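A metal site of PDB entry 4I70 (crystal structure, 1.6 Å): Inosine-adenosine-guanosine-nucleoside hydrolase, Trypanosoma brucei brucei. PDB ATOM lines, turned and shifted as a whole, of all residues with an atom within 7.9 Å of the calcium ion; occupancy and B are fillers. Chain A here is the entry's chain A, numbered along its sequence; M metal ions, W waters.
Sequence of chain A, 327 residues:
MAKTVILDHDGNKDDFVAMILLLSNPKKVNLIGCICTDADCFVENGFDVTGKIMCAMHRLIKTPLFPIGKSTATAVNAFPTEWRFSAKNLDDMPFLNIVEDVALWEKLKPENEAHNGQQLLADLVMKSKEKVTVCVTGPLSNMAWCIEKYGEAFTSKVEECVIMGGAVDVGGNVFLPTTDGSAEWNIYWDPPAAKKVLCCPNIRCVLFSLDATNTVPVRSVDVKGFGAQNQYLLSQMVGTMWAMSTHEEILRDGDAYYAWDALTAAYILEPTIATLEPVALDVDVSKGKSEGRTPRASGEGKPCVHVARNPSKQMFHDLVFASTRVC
ND2 of Asn 186 sits close to O of Thr 137 (3.2 Å). The backbone carbonyl oxygen (O) of Asp 10 sits close to the side-chain sulfur (SG) of Cys 41, at 3.3 Å. The backbone carbonyl oxygen (O) of Asp 8 is in hydrogen-bond range of the backbone NH (N) of Thr 137 (2.9 Å). The backbone NH (N) of Asp 40 lies within hydrogen-bond range of the side-chain carboxylate (OD2) of Asp 10, at 2.9 Å. OD2 of Asp 15 sits close to N of Asn 12 (2.9 Å).
Four residues have an atom within 4 Å of the calcium ion: Asp 10, Asp 15, Thr 137 and Asp 261. The nearest printed residue that does not touch the calcium ion is Gly 138 (4.2 Å).
The calcium ion is bound by O of Thr 137, OD1 of Asp 10, water W1, OD2 of Asp 261, OD2 of Asp 15, water W3, OD1 of Asp 15 and water W2. The calcium ion has eight donor atoms within binding distance.
Water W3 lies within hydrogen-bond range of OD2 of Asp 10 (2.7 Å) and OD1 of Asn 186 (2.7 Å). Water W2 lies within hydrogen-bond range of the side-chain carboxylate (OD1) of Asp 261 (2.7 Å) and the side-chain amide nitrogen (ND2) of Asn 186 (3.1 Å).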
ATOM      1  N   ASP A   8      25.034  11.896 -31.632  1.00  0.00           N
ATOM      2  CA  ASP A   8      24.129  12.561 -30.687  1.00  0.00           C
ATOM      3  C   ASP A   8      22.973  11.558 -30.497  1.00  0.00           C
ATOM      4  O   ASP A   8      22.115  11.434 -31.342  1.00  0.00           O
ATOM      5  CB  ASP A   8      23.737  13.890 -31.340  1.00  0.00           C
ATOM      6  CG  ASP A   8      22.690  14.668 -30.622  1.00  0.00           C
ATOM      7  OD1 ASP A   8      22.200  14.281 -29.541  1.00  0.00           O
ATOM      8  OD2 ASP A   8      22.312  15.739 -31.180  1.00  0.00           O
ATOM      9  N   HIS A   9      23.043  10.823 -29.403  1.00  0.00           N
ATOM     10  CA  HIS A   9      22.181   9.668 -29.158  1.00  0.00           C
ATOM     11  C   HIS A   9      21.448   9.689 -27.809  1.00  0.00           C
ATOM     12  O   HIS A   9      21.704  10.540 -26.970  1.00  0.00           O
ATOM     13  CB  HIS A   9      22.992   8.389 -29.318  1.00  0.00           C
ATOM     14  CG  HIS A   9      23.921   8.086 -28.176  1.00  0.00           C
ATOM     15  ND1 HIS A   9      23.471   7.514 -27.007  1.00  0.00           N
ATOM     16  CD2 HIS A   9      25.249   8.233 -28.048  1.00  0.00           C
ATOM     17  CE1 HIS A   9      24.498   7.340 -26.187  1.00  0.00           C
ATOM     18  NE2 HIS A   9      25.590   7.767 -26.794  1.00  0.00           N
ATOM     19  N   ASP A  10      20.540   8.734 -27.604  1.00  0.00           N
ATOM     20  CA  ASP A  10      19.799   8.673 -26.331  1.00  0.00           C
ATOM     21  C   ASP A  10      19.808   7.271 -25.735  1.00  0.00           C
ATOM     22  O   ASP A  10      18.925   6.862 -25.012  1.00  0.00           O
ATOM     23  CB  ASP A  10      18.399   9.263 -26.433  1.00  0.00           C
ATOM     24  CG  ASP A  10      17.478   8.429 -27.280  1.00  0.00           C
ATOM     25  OD1 ASP A  10      17.974   7.650 -28.114  1.00  0.00           O
ATOM     26  OD2 ASP A  10      16.241   8.614 -27.113  1.00  0.00           O
ATOM     27  N   GLY A  11      20.850   6.516 -26.047  1.00  0.00           N
ATOM     28  CA  GLY A  11      21.277   5.425 -25.186  1.00  0.00           C
ATOM     29  C   GLY A  11      20.411   4.191 -25.139  1.00  0.00           C
ATOM     30  O   GLY A  11      20.438   3.486 -24.126  1.00  0.00           O
ATOM     31  N   ASN A  12      19.642   3.922 -26.176  1.00  0.00           N
ATOM     32  CA  ASN A  12      18.952   2.629 -26.236  1.00  0.00           C
ATOM     33  C   ASN A  12      19.755   1.674 -27.131  1.00  0.00           C
ATOM     34  O   ASN A  12      20.819   2.035 -27.639  1.00  0.00           O
ATOM     35  CB  ASN A  12      17.491   2.790 -26.681  1.00  0.00           C
ATOM     36  CG  ASN A  12      16.565   1.737 -25.997  1.00  0.00           C
ATOM     37  OD1 ASN A  12      16.631   0.553 -26.300  1.00  0.00           O
ATOM     38  ND2 ASN A  12      15.787   2.187 -24.993  1.00  0.00           N
ATOM     39  N   LYS A  13      19.272   0.449 -27.278  1.00  0.00           N
ATOM     40  CA  LYS A  13      20.007  -0.600 -27.960  1.00  0.00           C
ATOM     41  C   LYS A  13      20.413  -0.186 -29.378  1.00  0.00           C
ATOM     42  O   LYS A  13      21.541  -0.407 -29.819  1.00  0.00           O
ATOM     43  CB  LYS A  13      19.155  -1.897 -28.010  1.00  0.00           C
ATOM     44  CG  LYS A  13      18.816  -2.421 -26.683  1.00  0.00           C
ATOM     45  CD  LYS A  13      17.876  -3.659 -26.695  1.00  0.00           C
ATOM     46  CE  LYS A  13      16.572  -3.524 -27.462  1.00  0.00           C
ATOM     47  NZ  LYS A  13      16.666  -4.132 -28.847  1.00  0.00           N
ATOM     48  N   ASP A  14      19.484   0.417 -30.116  1.00  0.00           N
ATOM     49  CA  ASP A  14      19.766   0.777 -31.483  1.00  0.00           C
ATOM     50  C   ASP A  14      20.743   1.922 -31.577  1.00  0.00           C
ATOM     51  O   ASP A  14      21.526   1.977 -32.499  1.00  0.00           O
ATOM     52  CB  ASP A  14      18.462   1.072 -32.229  1.00  0.00           C
ATOM     53  CG  ASP A  14      17.484  -0.092 -32.112  1.00  0.00           C
ATOM     54  OD1 ASP A  14      17.896  -1.222 -32.475  1.00  0.00           O
ATOM     55  OD2 ASP A  14      16.339   0.110 -31.598  1.00  0.00           O
ATOM     56  N   ASP A  15      20.750   2.792 -30.590  1.00  0.00           N
ATOM     57  CA  ASP A  15      21.756   3.845 -30.538  1.00  0.00           C
ATOM     58  C   ASP A  15      23.139   3.263 -30.469  1.00  0.00           C
ATOM     59  O   ASP A  15      24.074   3.760 -31.147  1.00  0.00           O
ATOM     60  CB  ASP A  15      21.525   4.744 -29.331  1.00  0.00           C
ATOM     61  CG  ASP A  15      20.172   5.459 -29.373  1.00  0.00           C
ATOM     62  OD1 ASP A  15      20.073   6.629 -29.862  1.00  0.00           O
ATOM     63  OD2 ASP A  15      19.171   4.833 -28.936  1.00  0.00           O
ATOM     64  N   PHE A  16      23.299   2.211 -29.673  1.00  0.00           N
ATOM     65  CA  PHE A  16      24.617   1.600 -29.542  1.00  0.00           C
ATOM     66  C   PHE A  16      25.024   0.766 -30.738  1.00  0.00           C
ATOM     67  O   PHE A  16      26.199   0.722 -31.054  1.00  0.00           O
ATOM     68  CB  PHE A  16      24.743   0.864 -28.219  1.00  0.00           C
ATOM     69  CG  PHE A  16      24.647   1.810 -27.067  1.00  0.00           C
ATOM     70  CD1 PHE A  16      25.596   2.836 -26.940  1.00  0.00           C
ATOM     71  CD2 PHE A  16      23.633   1.719 -26.138  1.00  0.00           C
ATOM     72  CE1 PHE A  16      25.533   3.728 -25.877  1.00  0.00           C
ATOM     73  CE2 PHE A  16      23.579   2.619 -25.069  1.00  0.00           C
ATOM     74  CZ  PHE A  16      24.514   3.624 -24.983  1.00  0.00           C
ATOM     75  N   ALA A  39      16.588  10.654 -22.812  1.00  0.00           N
ATOM     76  CA  ALA A  39      15.321  10.430 -23.547  1.00  0.00           C
ATOM     77  C   ALA A  39      14.954   8.987 -23.449  1.00  0.00           C
ATOM     78  O   ALA A  39      14.312   8.602 -22.465  1.00  0.00           O
ATOM     79  CB  ALA A  39      15.381  10.982 -25.011  1.00  0.00           C
ATOM     80  N   ASP A  40      15.364   8.139 -24.390  1.00  0.00           N
ATOM     81  CA  ASP A  40      15.057   6.685 -24.283  1.00  0.00           C
ATOM     82  C   ASP A  40      16.078   5.888 -23.472  1.00  0.00           C
ATOM     83  O   ASP A  40      16.386   4.739 -23.795  1.00  0.00           O
ATOM     84  CB  ASP A  40      14.921   6.072 -25.688  1.00  0.00           C
ATOM     85  CG  ASP A  40      14.063   4.835 -25.718  1.00  0.00           C
ATOM     86  OD1 ASP A  40      13.416   4.490 -24.704  1.00  0.00           O
ATOM     87  OD2 ASP A  40      14.046   4.213 -26.820  1.00  0.00           O
ATOM     88  N   CYS A  41      16.583   6.522 -22.415  1.00  0.00           N
ATOM     89  CA  CYS A  41      17.476   5.915 -21.444  1.00  0.00           C
ATOM     90  C   CYS A  41      17.424   6.757 -20.179  1.00  0.00           C
ATOM     91  O   CYS A  41      16.830   7.859 -20.164  1.00  0.00           O
ATOM     92  CB  CYS A  41      18.933   5.864 -21.935  1.00  0.00           C
ATOM     93  SG  CYS A  41      19.828   7.458 -21.870  1.00  0.00           S
ATOM     94  N   PHE A  79       9.734   9.448 -22.743  1.00  0.00           N
ATOM     95  CA  PHE A  79       9.564   8.071 -23.184  1.00  0.00           C
ATOM     96  C   PHE A  79       8.917   7.266 -22.041  1.00  0.00           C
ATOM     97  O   PHE A  79       9.043   7.636 -20.885  1.00  0.00           O
ATOM     98  CB  PHE A  79      10.897   7.419 -23.548  1.00  0.00           C
ATOM     99  CG  PHE A  79      11.350   7.685 -24.962  1.00  0.00           C
ATOM    100  CD1 PHE A  79      11.034   6.801 -25.969  1.00  0.00           C
ATOM    101  CD2 PHE A  79      12.082   8.803 -25.283  1.00  0.00           C
ATOM    102  CE1 PHE A  79      11.448   7.037 -27.283  1.00  0.00           C
ATOM    103  CE2 PHE A  79      12.484   9.047 -26.591  1.00  0.00           C
ATOM    104  CZ  PHE A  79      12.177   8.151 -27.581  1.00  0.00           C
ATOM    105  N   VAL A 136      22.208  11.819 -35.595  1.00  0.00           N
ATOM    106  CA  VAL A 136      21.249  12.060 -34.498  1.00  0.00           C
ATOM    107  C   VAL A 136      20.301  10.884 -34.374  1.00  0.00           C
ATOM    108  O   VAL A 136      19.516  10.634 -35.272  1.00  0.00           O
ATOM    109  CB  VAL A 136      20.454  13.390 -34.688  1.00  0.00           C
ATOM    110  CG1 VAL A 136      19.474  13.611 -33.482  1.00  0.00           C
ATOM    111  CG2 VAL A 136      21.390  14.589 -34.895  1.00  0.00           C
ATOM    112  N   THR A 137      20.432  10.131 -33.278  1.00  0.00           N
ATOM    113  CA  THR A 137      19.626   8.930 -33.063  1.00  0.00           C
ATOM    114  C   THR A 137      18.690   9.055 -31.838  1.00  0.00           C
ATOM    115  O   THR A 137      17.911   8.144 -31.552  1.00  0.00           O
ATOM    116  CB  THR A 137      20.507   7.671 -32.951  1.00  0.00           C
ATOM    117  OG1 THR A 137      21.386   7.804 -31.846  1.00  0.00           O
ATOM    118  CG2 THR A 137      21.312   7.483 -34.232  1.00  0.00           C
ATOM    119  N   GLY A 138      18.764  10.187 -31.138  1.00  0.00           N
ATOM    120  CA  GLY A 138      17.740  10.533 -30.141  1.00  0.00           C
ATOM    121  C   GLY A 138      16.967  11.766 -30.668  1.00  0.00           C
ATOM    122  O   GLY A 138      16.952  12.051 -31.873  1.00  0.00           O
ATOM    123  N   PRO A 139      16.326  12.505 -29.774  1.00  0.00           N
ATOM    124  CA  PRO A 139      15.617  13.719 -30.146  1.00  0.00           C
ATOM    125  C   PRO A 139      16.551  14.832 -30.658  1.00  0.00           C
ATOM    126  O   PRO A 139      17.754  14.780 -30.488  1.00  0.00           O
ATOM    127  CB  PRO A 139      14.898  14.102 -28.824  1.00  0.00           C
ATOM    128  CG  PRO A 139      14.726  12.811 -28.106  1.00  0.00           C
ATOM    129  CD  PRO A 139      16.041  12.136 -28.376  1.00  0.00           C
ATOM    130  N   MET A 164      17.477  10.001 -37.227  1.00  0.00           N
ATOM    131  CA  MET A 164      16.408   9.006 -37.100  1.00  0.00           C
ATOM    132  C   MET A 164      15.214   9.708 -36.474  1.00  0.00           C
ATOM    133  O   MET A 164      15.284  10.229 -35.345  1.00  0.00           O
ATOM    134  CB  MET A 164      16.844   7.804 -36.272  1.00  0.00           C
ATOM    135  CG  MET A 164      15.921   6.593 -36.450  1.00  0.00           C
ATOM    136  SD  MET A 164      14.380   6.820 -35.555  1.00  0.00           S
ATOM    137  CE  MET A 164      13.289   5.714 -36.457  1.00  0.00           C
ATOM    138  N   GLU A 184       6.120  10.020 -34.540  1.00  0.00           N
ATOM    139  CA  GLU A 184       7.256   9.156 -34.187  1.00  0.00           C
ATOM    140  C   GLU A 184       7.936   9.689 -32.931  1.00  0.00           C
ATOM    141  O   GLU A 184       8.007  10.910 -32.703  1.00  0.00           O
ATOM    142  CB  GLU A 184       8.180   9.020 -35.383  1.00  0.00           C
ATOM    143  CG  GLU A 184       9.400   8.182 -35.168  1.00  0.00           C
ATOM    144  CD  GLU A 184      10.508   8.902 -34.419  1.00  0.00           C
ATOM    145  OE1 GLU A 184      10.596  10.140 -34.529  1.00  0.00           O
ATOM    146  OE2 GLU A 184      11.297   8.233 -33.753  1.00  0.00           O
ATOM    147  N   ASN A 186      11.052  10.075 -31.492  1.00  0.00           N
ATOM    148  CA  ASN A 186      12.138  11.072 -31.402  1.00  0.00           C
ATOM    149  C   ASN A 186      11.652  12.502 -31.620  1.00  0.00           C
ATOM    150  O   ASN A 186      12.113  13.404 -30.929  1.00  0.00           O
ATOM    151  CB  ASN A 186      13.298  10.717 -32.346  1.00  0.00           C
ATOM    152  CG  ASN A 186      14.138   9.564 -31.830  1.00  0.00           C
ATOM    153  OD1 ASN A 186      13.995   9.150 -30.683  1.00  0.00           O
ATOM    154  ND2 ASN A 186      15.098   9.106 -32.639  1.00  0.00           N
ATOM    155  N   TRP A 260      16.015   0.742 -37.414  1.00  0.00           N
ATOM    156  CA  TRP A 260      15.879   2.053 -36.806  1.00  0.00           C
ATOM    157  C   TRP A 260      17.197   2.846 -36.804  1.00  0.00           C
ATOM    158  O   TRP A 260      17.753   3.121 -37.877  1.00  0.00           O
ATOM    159  CB  TRP A 260      15.214   1.893 -35.439  1.00  0.00           C
ATOM    160  CG  TRP A 260      13.772   1.480 -35.500  1.00  0.00           C
ATOM    161  CD1 TRP A 260      12.789   1.975 -36.337  1.00  0.00           C
ATOM    162  CD2 TRP A 260      13.139   0.502 -34.677  1.00  0.00           C
ATOM    163  NE1 TRP A 260      11.582   1.356 -36.048  1.00  0.00           N
ATOM    164  CE2 TRP A 260      11.783   0.433 -35.049  1.00  0.00           C
ATOM    165  CE3 TRP A 260      13.594  -0.327 -33.640  1.00  0.00           C
ATOM    166  CZ2 TRP A 260      10.866  -0.436 -34.440  1.00  0.00           C
ATOM    167  CZ3 TRP A 260      12.668  -1.205 -33.038  1.00  0.00           C
ATOM    168  CH2 TRP A 260      11.332  -1.226 -33.436  1.00  0.00           C
ATOM    169  N   ASP A 261      17.682   3.238 -35.630  1.00  0.00           N
ATOM    170  CA  ASP A 261      18.829   4.143 -35.506  1.00  0.00           C
ATOM    171  C   ASP A 261      20.075   3.654 -36.256  1.00  0.00           C
ATOM    172  O   ASP A 261      20.897   4.458 -36.695  1.00  0.00           O
ATOM    173  CB  ASP A 261      19.263   4.324 -34.043  1.00  0.00           C
ATOM    174  CG  ASP A 261      18.114   4.572 -33.055  1.00  0.00           C
ATOM    175  OD1 ASP A 261      16.926   4.248 -33.357  1.00  0.00           O
ATOM    176  OD2 ASP A 261      18.430   5.009 -31.921  1.00  0.00           O
HETATM  177 CA    CA M   1      17.514   6.323 -30.083  1.00  0.00          CA
HETATM  178  O   HOH W   1      16.204   4.389 -29.416  1.00  0.00           O
HETATM  179  O   HOH W   2      15.667   6.186 -31.911  1.00  0.00           O
HETATM  180  O   HOH W   3      15.356   7.338 -29.261  1.00  0.00           O
